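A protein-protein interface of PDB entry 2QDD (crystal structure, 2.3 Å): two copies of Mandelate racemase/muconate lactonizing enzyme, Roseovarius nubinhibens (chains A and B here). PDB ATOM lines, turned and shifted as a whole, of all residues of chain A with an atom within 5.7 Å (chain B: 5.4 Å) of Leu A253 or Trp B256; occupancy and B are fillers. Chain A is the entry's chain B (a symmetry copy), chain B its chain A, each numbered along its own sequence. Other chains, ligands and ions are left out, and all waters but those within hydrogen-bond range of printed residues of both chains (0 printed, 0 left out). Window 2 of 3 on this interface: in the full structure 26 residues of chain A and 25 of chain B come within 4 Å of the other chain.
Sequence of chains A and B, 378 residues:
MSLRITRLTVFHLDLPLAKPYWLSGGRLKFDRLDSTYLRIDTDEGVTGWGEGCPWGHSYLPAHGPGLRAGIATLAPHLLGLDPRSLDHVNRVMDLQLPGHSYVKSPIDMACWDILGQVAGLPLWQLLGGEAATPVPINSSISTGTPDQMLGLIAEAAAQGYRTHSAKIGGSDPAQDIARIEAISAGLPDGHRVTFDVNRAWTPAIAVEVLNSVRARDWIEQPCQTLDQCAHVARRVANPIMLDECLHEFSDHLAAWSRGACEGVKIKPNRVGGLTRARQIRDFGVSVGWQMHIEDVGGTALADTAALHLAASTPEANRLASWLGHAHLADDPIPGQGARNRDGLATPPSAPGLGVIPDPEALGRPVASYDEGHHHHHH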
ATOM      1  N   PHE A 249     -12.780 -28.189 -28.872  1.00  0.00           N
ATOM      2  CA  PHE A 249     -13.604 -27.064 -28.430  1.00  0.00           C
ATOM      3  C   PHE A 249     -14.311 -26.336 -29.583  1.00  0.00           C
ATOM      4  O   PHE A 249     -15.451 -25.883 -29.433  1.00  0.00           O
ATOM      5  CB  PHE A 249     -12.763 -26.077 -27.603  1.00  0.00           C
ATOM      6  CG  PHE A 249     -13.557 -24.932 -27.033  1.00  0.00           C
ATOM      7  CD1 PHE A 249     -14.419 -25.134 -25.957  1.00  0.00           C
ATOM      8  CD2 PHE A 249     -13.459 -23.654 -27.587  1.00  0.00           C
ATOM      9  CE1 PHE A 249     -15.165 -24.079 -25.435  1.00  0.00           C
ATOM     10  CE2 PHE A 249     -14.197 -22.594 -27.073  1.00  0.00           C
ATOM     11  CZ  PHE A 249     -15.053 -22.808 -25.993  1.00  0.00           C
ATOM     12  N   SER A 250     -13.635 -26.240 -30.727  1.00  0.00           N
ATOM     13  CA  SER A 250     -14.187 -25.587 -31.917  1.00  0.00           C
ATOM     14  C   SER A 250     -15.422 -26.286 -32.494  1.00  0.00           C
ATOM     15  O   SER A 250     -16.274 -25.634 -33.094  1.00  0.00           O
ATOM     16  CB  SER A 250     -13.112 -25.425 -32.997  1.00  0.00           C
ATOM     17  OG  SER A 250     -12.766 -26.664 -33.588  1.00  0.00           O
ATOM     18  N   ASP A 251     -15.513 -27.602 -32.297  1.00  0.00           N
ATOM     19  CA  ASP A 251     -16.694 -28.382 -32.687  1.00  0.00           C
ATOM     20  C   ASP A 251     -17.885 -28.054 -31.806  1.00  0.00           C
ATOM     21  O   ASP A 251     -19.021 -28.060 -32.276  1.00  0.00           O
ATOM     22  CB  ASP A 251     -16.402 -29.883 -32.615  1.00  0.00           C
ATOM     23  CG  ASP A 251     -15.366 -30.334 -33.637  1.00  0.00           C
ATOM     24  OD1 ASP A 251     -14.487 -31.144 -33.273  1.00  0.00           O
ATOM     25  OD2 ASP A 251     -15.434 -29.888 -34.806  1.00  0.00           O
ATOM     26  N   HIS A 252     -17.615 -27.769 -30.531  1.00  0.00           N
ATOM     27  CA  HIS A 252     -18.651 -27.388 -29.573  1.00  0.00           C
ATOM     28  C   HIS A 252     -19.175 -25.985 -29.855  1.00  0.00           C
ATOM     29  O   HIS A 252     -20.380 -25.750 -29.803  1.00  0.00           O
ATOM     30  CB  HIS A 252     -18.129 -27.496 -28.138  1.00  0.00           C
ATOM     31  CG  HIS A 252     -17.775 -28.892 -27.733  1.00  0.00           C
ATOM     32  ND1 HIS A 252     -16.573 -29.480 -28.062  1.00  0.00           N
ATOM     33  CD2 HIS A 252     -18.474 -29.827 -27.045  1.00  0.00           C
ATOM     34  CE1 HIS A 252     -16.545 -30.716 -27.595  1.00  0.00           C
ATOM     35  NE2 HIS A 252     -17.684 -30.949 -26.969  1.00  0.00           N
ATOM     36  N   LEU A 253     -18.253 -25.070 -30.152  1.00  0.00           N
ATOM     37  CA  LEU A 253     -18.553 -23.717 -30.633  1.00  0.00           C
ATOM     38  C   LEU A 253     -19.422 -23.714 -31.895  1.00  0.00           C
ATOM     39  O   LEU A 253     -20.422 -23.001 -31.956  1.00  0.00           O
ATOM     40  CB  LEU A 253     -17.233 -23.002 -30.924  1.00  0.00           C
ATOM     41  CG  LEU A 253     -16.990 -21.534 -30.579  1.00  0.00           C
ATOM     42  CD1 LEU A 253     -17.801 -21.040 -29.389  1.00  0.00           C
ATOM     43  CD2 LEU A 253     -15.511 -21.339 -30.346  1.00  0.00           C
ATOM     44  N   ALA A 254     -19.036 -24.519 -32.887  1.00  0.00           N
ATOM     45  CA  ALA A 254     -19.830 -24.727 -34.108  1.00  0.00           C
ATOM     46  C   ALA A 254     -21.229 -25.298 -33.841  1.00  0.00           C
ATOM     47  O   ALA A 254     -22.192 -24.887 -34.481  1.00  0.00           O
ATOM     48  CB  ALA A 254     -19.079 -25.625 -35.086  1.00  0.00           C
ATOM     49  N   ALA A 255     -21.329 -26.232 -32.896  1.00  0.00           N
ATOM     50  CA  ALA A 255     -22.612 -26.829 -32.515  1.00  0.00           C
ATOM     51  C   ALA A 255     -23.546 -25.798 -31.890  1.00  0.00           C
ATOM     52  O   ALA A 255     -24.741 -25.770 -32.188  1.00  0.00           O
ATOM     53  CB  ALA A 255     -22.396 -28.001 -31.555  1.00  0.00           C
ATOM     54  N   TRP A 256     -22.991 -24.956 -31.023  1.00  0.00           N
ATOM     55  CA  TRP A 256     -23.763 -23.916 -30.365  1.00  0.00           C
ATOM     56  C   TRP A 256     -24.263 -22.879 -31.382  1.00  0.00           C
ATOM     57  O   TRP A 256     -25.430 -22.489 -31.339  1.00  0.00           O
ATOM     58  CB  TRP A 256     -22.954 -23.258 -29.236  1.00  0.00           C
ATOM     59  CG  TRP A 256     -23.584 -21.992 -28.751  1.00  0.00           C
ATOM     60  CD1 TRP A 256     -24.615 -21.879 -27.862  1.00  0.00           C
ATOM     61  CD2 TRP A 256     -23.266 -20.657 -29.172  1.00  0.00           C
ATOM     62  NE1 TRP A 256     -24.950 -20.557 -27.692  1.00  0.00           N
ATOM     63  CE2 TRP A 256     -24.142 -19.786 -28.488  1.00  0.00           C
ATOM     64  CE3 TRP A 256     -22.330 -20.116 -30.066  1.00  0.00           C
ATOM     65  CZ2 TRP A 256     -24.104 -18.399 -28.655  1.00  0.00           C
ATOM     66  CZ3 TRP A 256     -22.291 -18.730 -30.239  1.00  0.00           C
ATOM     67  CH2 TRP A 256     -23.176 -17.890 -29.537  1.00  0.00           C
ATOM     68  N   SER A 257     -23.385 -22.448 -32.293  1.00  0.00           N
ATOM     69  CA  SER A 257     -23.738 -21.439 -33.301  1.00  0.00           C
ATOM     70  C   SER A 257     -24.747 -21.922 -34.354  1.00  0.00           C
ATOM     71  O   SER A 257     -25.509 -21.117 -34.889  1.00  0.00           O
ATOM     72  CB  SER A 257     -22.489 -20.867 -33.977  1.00  0.00           C
ATOM     73  OG  SER A 257     -21.850 -21.845 -34.770  1.00  0.00           O
ATOM     74  N   ARG A 258     -24.732 -23.230 -34.635  1.00  0.00           N
ATOM     75  CA  ARG A 258     -25.718 -23.891 -35.498  1.00  0.00           C
ATOM     76  C   ARG A 258     -27.050 -24.123 -34.779  1.00  0.00           C
ATOM     77  O   ARG A 258     -28.080 -24.330 -35.418  1.00  0.00           O
ATOM     78  CB  ARG A 258     -25.189 -25.254 -35.949  1.00  0.00           C
ATOM     79  CG  ARG A 258     -24.330 -25.261 -37.195  1.00  0.00           C
ATOM     80  CD  ARG A 258     -23.947 -26.695 -37.525  1.00  0.00           C
ATOM     81  NE  ARG A 258     -23.222 -26.829 -38.787  1.00  0.00           N
ATOM     82  CZ  ARG A 258     -23.790 -27.084 -39.964  1.00  0.00           C
ATOM     83  NH1 ARG A 258     -25.108 -27.226 -40.065  1.00  0.00           N
ATOM     84  NH2 ARG A 258     -23.034 -27.194 -41.046  1.00  0.00           N
ATOM     85  N   PHE A 283     -18.071 -23.783 -20.740  1.00  0.00           N
ATOM     86  CA  PHE A 283     -18.816 -23.281 -21.903  1.00  0.00           C
ATOM     87  C   PHE A 283     -20.270 -23.754 -21.896  1.00  0.00           C
ATOM     88  O   PHE A 283     -21.179 -22.960 -22.128  1.00  0.00           O
ATOM     89  CB  PHE A 283     -18.144 -23.695 -23.224  1.00  0.00           C
ATOM     90  CG  PHE A 283     -18.921 -23.292 -24.451  1.00  0.00           C
ATOM     91  CD1 PHE A 283     -19.734 -24.208 -25.116  1.00  0.00           C
ATOM     92  CD2 PHE A 283     -18.844 -21.987 -24.939  1.00  0.00           C
ATOM     93  CE1 PHE A 283     -20.458 -23.832 -26.253  1.00  0.00           C
ATOM     94  CE2 PHE A 283     -19.564 -21.602 -26.074  1.00  0.00           C
ATOM     95  CZ  PHE A 283     -20.367 -22.525 -26.729  1.00  0.00           C
ATOM     96  N   TRP A 289     -26.424 -25.756 -21.669  1.00  0.00           N
ATOM     97  CA  TRP A 289     -26.427 -27.190 -21.970  1.00  0.00           C
ATOM     98  C   TRP A 289     -26.579 -28.034 -20.712  1.00  0.00           C
ATOM     99  O   TRP A 289     -26.115 -27.659 -19.638  1.00  0.00           O
ATOM    100  CB  TRP A 289     -25.160 -27.613 -22.709  1.00  0.00           C
ATOM    101  CG  TRP A 289     -25.101 -27.226 -24.161  1.00  0.00           C
ATOM    102  CD1 TRP A 289     -26.145 -26.863 -24.968  1.00  0.00           C
ATOM    103  CD2 TRP A 289     -23.930 -27.191 -24.983  1.00  0.00           C
ATOM    104  NE1 TRP A 289     -25.694 -26.593 -26.238  1.00  0.00           N
ATOM    105  CE2 TRP A 289     -24.338 -26.785 -26.276  1.00  0.00           C
ATOM    106  CE3 TRP A 289     -22.569 -27.457 -24.753  1.00  0.00           C
ATOM    107  CZ2 TRP A 289     -23.434 -26.642 -27.337  1.00  0.00           C
ATOM    108  CZ3 TRP A 289     -21.673 -27.312 -25.805  1.00  0.00           C
ATOM    109  CH2 TRP A 289     -22.113 -26.912 -27.085  1.00  0.00           C
ATOM    110  N   ASP B 251     -21.399 -11.759 -24.203  1.00  0.00           N
ATOM    111  CA  ASP B 251     -20.981 -10.635 -25.049  1.00  0.00           C
ATOM    112  C   ASP B 251     -19.753 -10.944 -25.896  1.00  0.00           C
ATOM    113  O   ASP B 251     -19.603 -10.400 -26.990  1.00  0.00           O
ATOM    114  CB  ASP B 251     -20.724  -9.376 -24.209  1.00  0.00           C
ATOM    115  CG  ASP B 251     -21.959  -8.913 -23.441  1.00  0.00           C
ATOM    116  OD1 ASP B 251     -21.790  -8.336 -22.344  1.00  0.00           O
ATOM    117  OD2 ASP B 251     -23.094  -9.122 -23.931  1.00  0.00           O
ATOM    118  N   HIS B 252     -18.873 -11.808 -25.382  1.00  0.00           N
ATOM    119  CA  HIS B 252     -17.672 -12.226 -26.104  1.00  0.00           C
ATOM    120  C   HIS B 252     -18.023 -13.232 -27.194  1.00  0.00           C
ATOM    121  O   HIS B 252     -17.519 -13.151 -28.322  1.00  0.00           O
ATOM    122  CB  HIS B 252     -16.639 -12.815 -25.139  1.00  0.00           C
ATOM    123  CG  HIS B 252     -16.118 -11.828 -24.145  1.00  0.00           C
ATOM    124  ND1 HIS B 252     -16.817 -11.475 -23.011  1.00  0.00           N
ATOM    125  CD2 HIS B 252     -14.979 -11.095 -24.131  1.00  0.00           C
ATOM    126  CE1 HIS B 252     -16.124 -10.579 -22.330  1.00  0.00           C
ATOM    127  NE2 HIS B 252     -15.006 -10.328 -22.990  1.00  0.00           N
ATOM    128  N   LEU B 253     -18.891 -14.174 -26.827  1.00  0.00           N
ATOM    129  CA  LEU B 253     -19.568 -15.087 -27.746  1.00  0.00           C
ATOM    130  C   LEU B 253     -20.289 -14.382 -28.893  1.00  0.00           C
ATOM    131  O   LEU B 253     -20.209 -14.820 -30.037  1.00  0.00           O
ATOM    132  CB  LEU B 253     -20.578 -15.922 -26.957  1.00  0.00           C
ATOM    133  CG  LEU B 253     -20.521 -17.445 -27.040  1.00  0.00           C
ATOM    134  CD1 LEU B 253     -19.103 -17.973 -26.890  1.00  0.00           C
ATOM    135  CD2 LEU B 253     -21.440 -18.050 -25.986  1.00  0.00           C
ATOM    136  N   ALA B 254     -20.992 -13.299 -28.566  1.00  0.00           N
ATOM    137  CA  ALA B 254     -21.623 -12.422 -29.550  1.00  0.00           C
ATOM    138  C   ALA B 254     -20.625 -11.722 -30.463  1.00  0.00           C
ATOM    139  O   ALA B 254     -20.829 -11.683 -31.675  1.00  0.00           O
ATOM    140  CB  ALA B 254     -22.517 -11.397 -28.854  1.00  0.00           C
ATOM    141  N   ALA B 255     -19.556 -11.173 -29.881  1.00  0.00           N
ATOM    142  CA  ALA B 255     -18.492 -10.516 -30.652  1.00  0.00           C
ATOM    143  C   ALA B 255     -17.839 -11.482 -31.637  1.00  0.00           C
ATOM    144  O   ALA B 255     -17.575 -11.124 -32.786  1.00  0.00           O
ATOM    145  CB  ALA B 255     -17.436  -9.920 -29.715  1.00  0.00           C
ATOM    146  N   TRP B 256     -17.603 -12.710 -31.175  1.00  0.00           N
ATOM    147  CA  TRP B 256     -17.003 -13.759 -31.993  1.00  0.00           C
ATOM    148  C   TRP B 256     -17.866 -14.162 -33.207  1.00  0.00           C
ATOM    149  O   TRP B 256     -17.359 -14.237 -34.330  1.00  0.00           O
ATOM    150  CB  TRP B 256     -16.649 -14.989 -31.139  1.00  0.00           C
ATOM    151  CG  TRP B 256     -16.207 -16.133 -31.981  1.00  0.00           C
ATOM    152  CD1 TRP B 256     -14.978 -16.301 -32.557  1.00  0.00           C
ATOM    153  CD2 TRP B 256     -17.004 -17.245 -32.401  1.00  0.00           C
ATOM    154  NE1 TRP B 256     -14.957 -17.463 -33.294  1.00  0.00           N
ATOM    155  CE2 TRP B 256     -16.189 -18.058 -33.220  1.00  0.00           C
ATOM    156  CE3 TRP B 256     -18.331 -17.632 -32.167  1.00  0.00           C
ATOM    157  CZ2 TRP B 256     -16.653 -19.244 -33.796  1.00  0.00           C
ATOM    158  CZ3 TRP B 256     -18.796 -18.812 -32.746  1.00  0.00           C
ATOM    159  CH2 TRP B 256     -17.957 -19.602 -33.552  1.00  0.00           C
ATOM    160  N   SER B 257     -19.152 -14.419 -32.972  1.00  0.00           N
ATOM    161  CA  SER B 257     -20.052 -14.884 -34.025  1.00  0.00           C
ATOM    162  C   SER B 257     -20.434 -13.817 -35.057  1.00  0.00           C
ATOM    163  O   SER B 257     -20.812 -14.153 -36.177  1.00  0.00           O
ATOM    164  CB  SER B 257     -21.302 -15.550 -33.437  1.00  0.00           C
ATOM    165  OG  SER B 257     -21.996 -14.668 -32.580  1.00  0.00           O
ATOM    166  N   ARG B 258     -20.330 -12.542 -34.678  1.00  0.00           N
ATOM    167  CA  ARG B 258     -20.516 -11.425 -35.611  1.00  0.00           C
ATOM    168  C   ARG B 258     -19.251 -11.117 -36.415  1.00  0.00           C
ATOM    169  O   ARG B 258     -19.314 -10.398 -37.408  1.00  0.00           O
ATOM    170  CB  ARG B 258     -20.945 -10.155 -34.871  1.00  0.00           C
ATOM    171  CG  ARG B 258     -22.357 -10.161 -34.327  1.00  0.00           C
ATOM    172  CD  ARG B 258     -22.482  -9.133 -33.212  1.00  0.00           C
ATOM    173  NE  ARG B 258     -23.869  -8.760 -32.936  1.00  0.00           N
ATOM    174  CZ  ARG B 258     -24.523  -7.775 -33.546  1.00  0.00           C
ATOM    175  NH1 ARG B 258     -25.782  -7.521 -33.218  1.00  0.00           N
ATOM    176  NH2 ARG B 258     -23.929  -7.047 -34.487  1.00  0.00           N
ATOM    177  N   GLY B 259     -18.109 -11.641 -35.975  1.00  0.00           N
ATOM    178  CA  GLY B 259     -16.803 -11.273 -36.539  1.00  0.00           C
ATOM    179  C   GLY B 259     -16.399  -9.830 -36.275  1.00  0.00           C
ATOM    180  O   GLY B 259     -15.790  -9.184 -37.124  1.00  0.00           O
ATOM    181  N   ALA B 260     -16.722  -9.340 -35.080  1.00  0.00           N
ATOM    182  CA  ALA B 260     -16.674  -7.915 -34.763  1.00  0.00           C
ATOM    183  C   ALA B 260     -15.273  -7.408 -34.454  1.00  0.00           C
ATOM    184  O   ALA B 260     -15.039  -6.199 -34.462  1.00  0.00           O
ATOM    185  CB  ALA B 260     -17.588  -7.613 -33.596  1.00  0.00           C
ATOM    186  N   PHE B 283     -11.138 -18.792 -23.980  1.00  0.00           N
ATOM    187  CA  PHE B 283     -11.949 -18.627 -25.183  1.00  0.00           C
ATOM    188  C   PHE B 283     -11.177 -17.877 -26.271  1.00  0.00           C
ATOM    189  O   PHE B 283     -11.157 -18.310 -27.421  1.00  0.00           O
ATOM    190  CB  PHE B 283     -13.277 -17.919 -24.874  1.00  0.00           C
ATOM    191  CG  PHE B 283     -14.138 -17.695 -26.090  1.00  0.00           C
ATOM    192  CD1 PHE B 283     -14.256 -16.430 -26.652  1.00  0.00           C
ATOM    193  CD2 PHE B 283     -14.827 -18.749 -26.672  1.00  0.00           C
ATOM    194  CE1 PHE B 283     -15.041 -16.216 -27.778  1.00  0.00           C
ATOM    195  CE2 PHE B 283     -15.617 -18.546 -27.800  1.00  0.00           C
ATOM    196  CZ  PHE B 283     -15.724 -17.280 -28.353  1.00  0.00           C
ATOM    197  N   VAL B 287      -9.960 -19.095 -30.232  1.00  0.00           N
ATOM    198  CA  VAL B 287     -10.479 -18.452 -31.446  1.00  0.00           C
ATOM    199  C   VAL B 287      -9.451 -17.523 -32.096  1.00  0.00           C
ATOM    200  O   VAL B 287      -9.714 -16.910 -33.138  1.00  0.00           O
ATOM    201  CB  VAL B 287     -11.840 -17.713 -31.200  1.00  0.00           C
ATOM    202  CG1 VAL B 287     -12.880 -18.668 -30.649  1.00  0.00           C
ATOM    203  CG2 VAL B 287     -11.678 -16.521 -30.265  1.00  0.00           C
ATOM    204  N   TRP B 289      -7.835 -14.768 -30.748  1.00  0.00           N
ATOM    205  CA  TRP B 289      -7.814 -13.360 -30.362  1.00  0.00           C
ATOM    206  C   TRP B 289      -6.452 -12.974 -29.801  1.00  0.00           C
ATOM    207  O   TRP B 289      -5.756 -13.798 -29.210  1.00  0.00           O
ATOM    208  CB  TRP B 289      -8.898 -13.064 -29.322  1.00  0.00           C
ATOM    209  CG  TRP B 289     -10.288 -12.900 -29.883  1.00  0.00           C
ATOM    210  CD1 TRP B 289     -10.637 -12.737 -31.193  1.00  0.00           C
ATOM    211  CD2 TRP B 289     -11.514 -12.868 -29.135  1.00  0.00           C
ATOM    212  NE1 TRP B 289     -12.002 -12.613 -31.309  1.00  0.00           N
ATOM    213  CE2 TRP B 289     -12.564 -12.686 -30.061  1.00  0.00           C
ATOM    214  CE3 TRP B 289     -11.825 -12.975 -27.772  1.00  0.00           C
ATOM    215  CZ2 TRP B 289     -13.911 -12.614 -29.668  1.00  0.00           C
ATOM    216  CZ3 TRP B 289     -13.165 -12.906 -27.383  1.00  0.00           C
ATOM    217  CH2 TRP B 289     -14.186 -12.722 -28.330  1.00  0.00           C
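The backbone carbonyl oxygen (O) of Leu B253 lies within hydrogen-bond range of the side-chain hydroxyl (OG) of Ser B257, 3.1 Å away. The backbone carbonyl oxygen of Leu A253 is in hydrogen-bond range of the side-chain hydroxyl of Ser A257.
Among the printed residues, merely in contact across the chains: Phe A249 with Phe B283 (3.9 Å), Leu A253 with Trp B256 (3.7 Å), Leu A253 with Phe B283 (3.7 Å), Leu A253 with Val B287 (3.8 Å), Trp A256 with Leu B253 (3.7 Å) and Phe A283 with Leu B253 (3.7 Å).
Of the printed residues of chain B, Phe A249 touches Phe B283. Leu A253 touches just these residues of chain B: Trp B256, Phe B283 and Val B287. Of the printed residues of chain B, Phe A283 touches Leu B253 (3.7 Å). Of chain A, only Leu A253 comes within 4 Å of Trp B256. Ala B260 touches none of the printed residues of chain A. The nearest residue of chain A that does not touch Trp B256 is Trp A256 (4.3 Å).
Printed residues of chain A that touch a printed residue of chain B: Phe A249, Leu A253, Trp A256 and Phe A283. Hydrophobic or aromatic side chains of chain A within 4 Å of the printed part of chain B: Phe A249, Leu A253, Trp A256 and Phe A283. Printed residues of chain B that touch a printed residue of chain A: Leu B253, Trp B256, Phe B283 and Val B287. Among the printed residues, 6 pairs touch across the chains.
Leu A253 touches Trp B256, and with the chains exchanged Trp A256 touches Leu B253. Leu A253 touches Phe B283, and with the chains exchanged Phe A283 touches Leu B253. 10 positions are printed for both chains. Of the 6 pairs that touch across the chains among the printed residues, 4 have their exchanged pair printed and touching as well.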
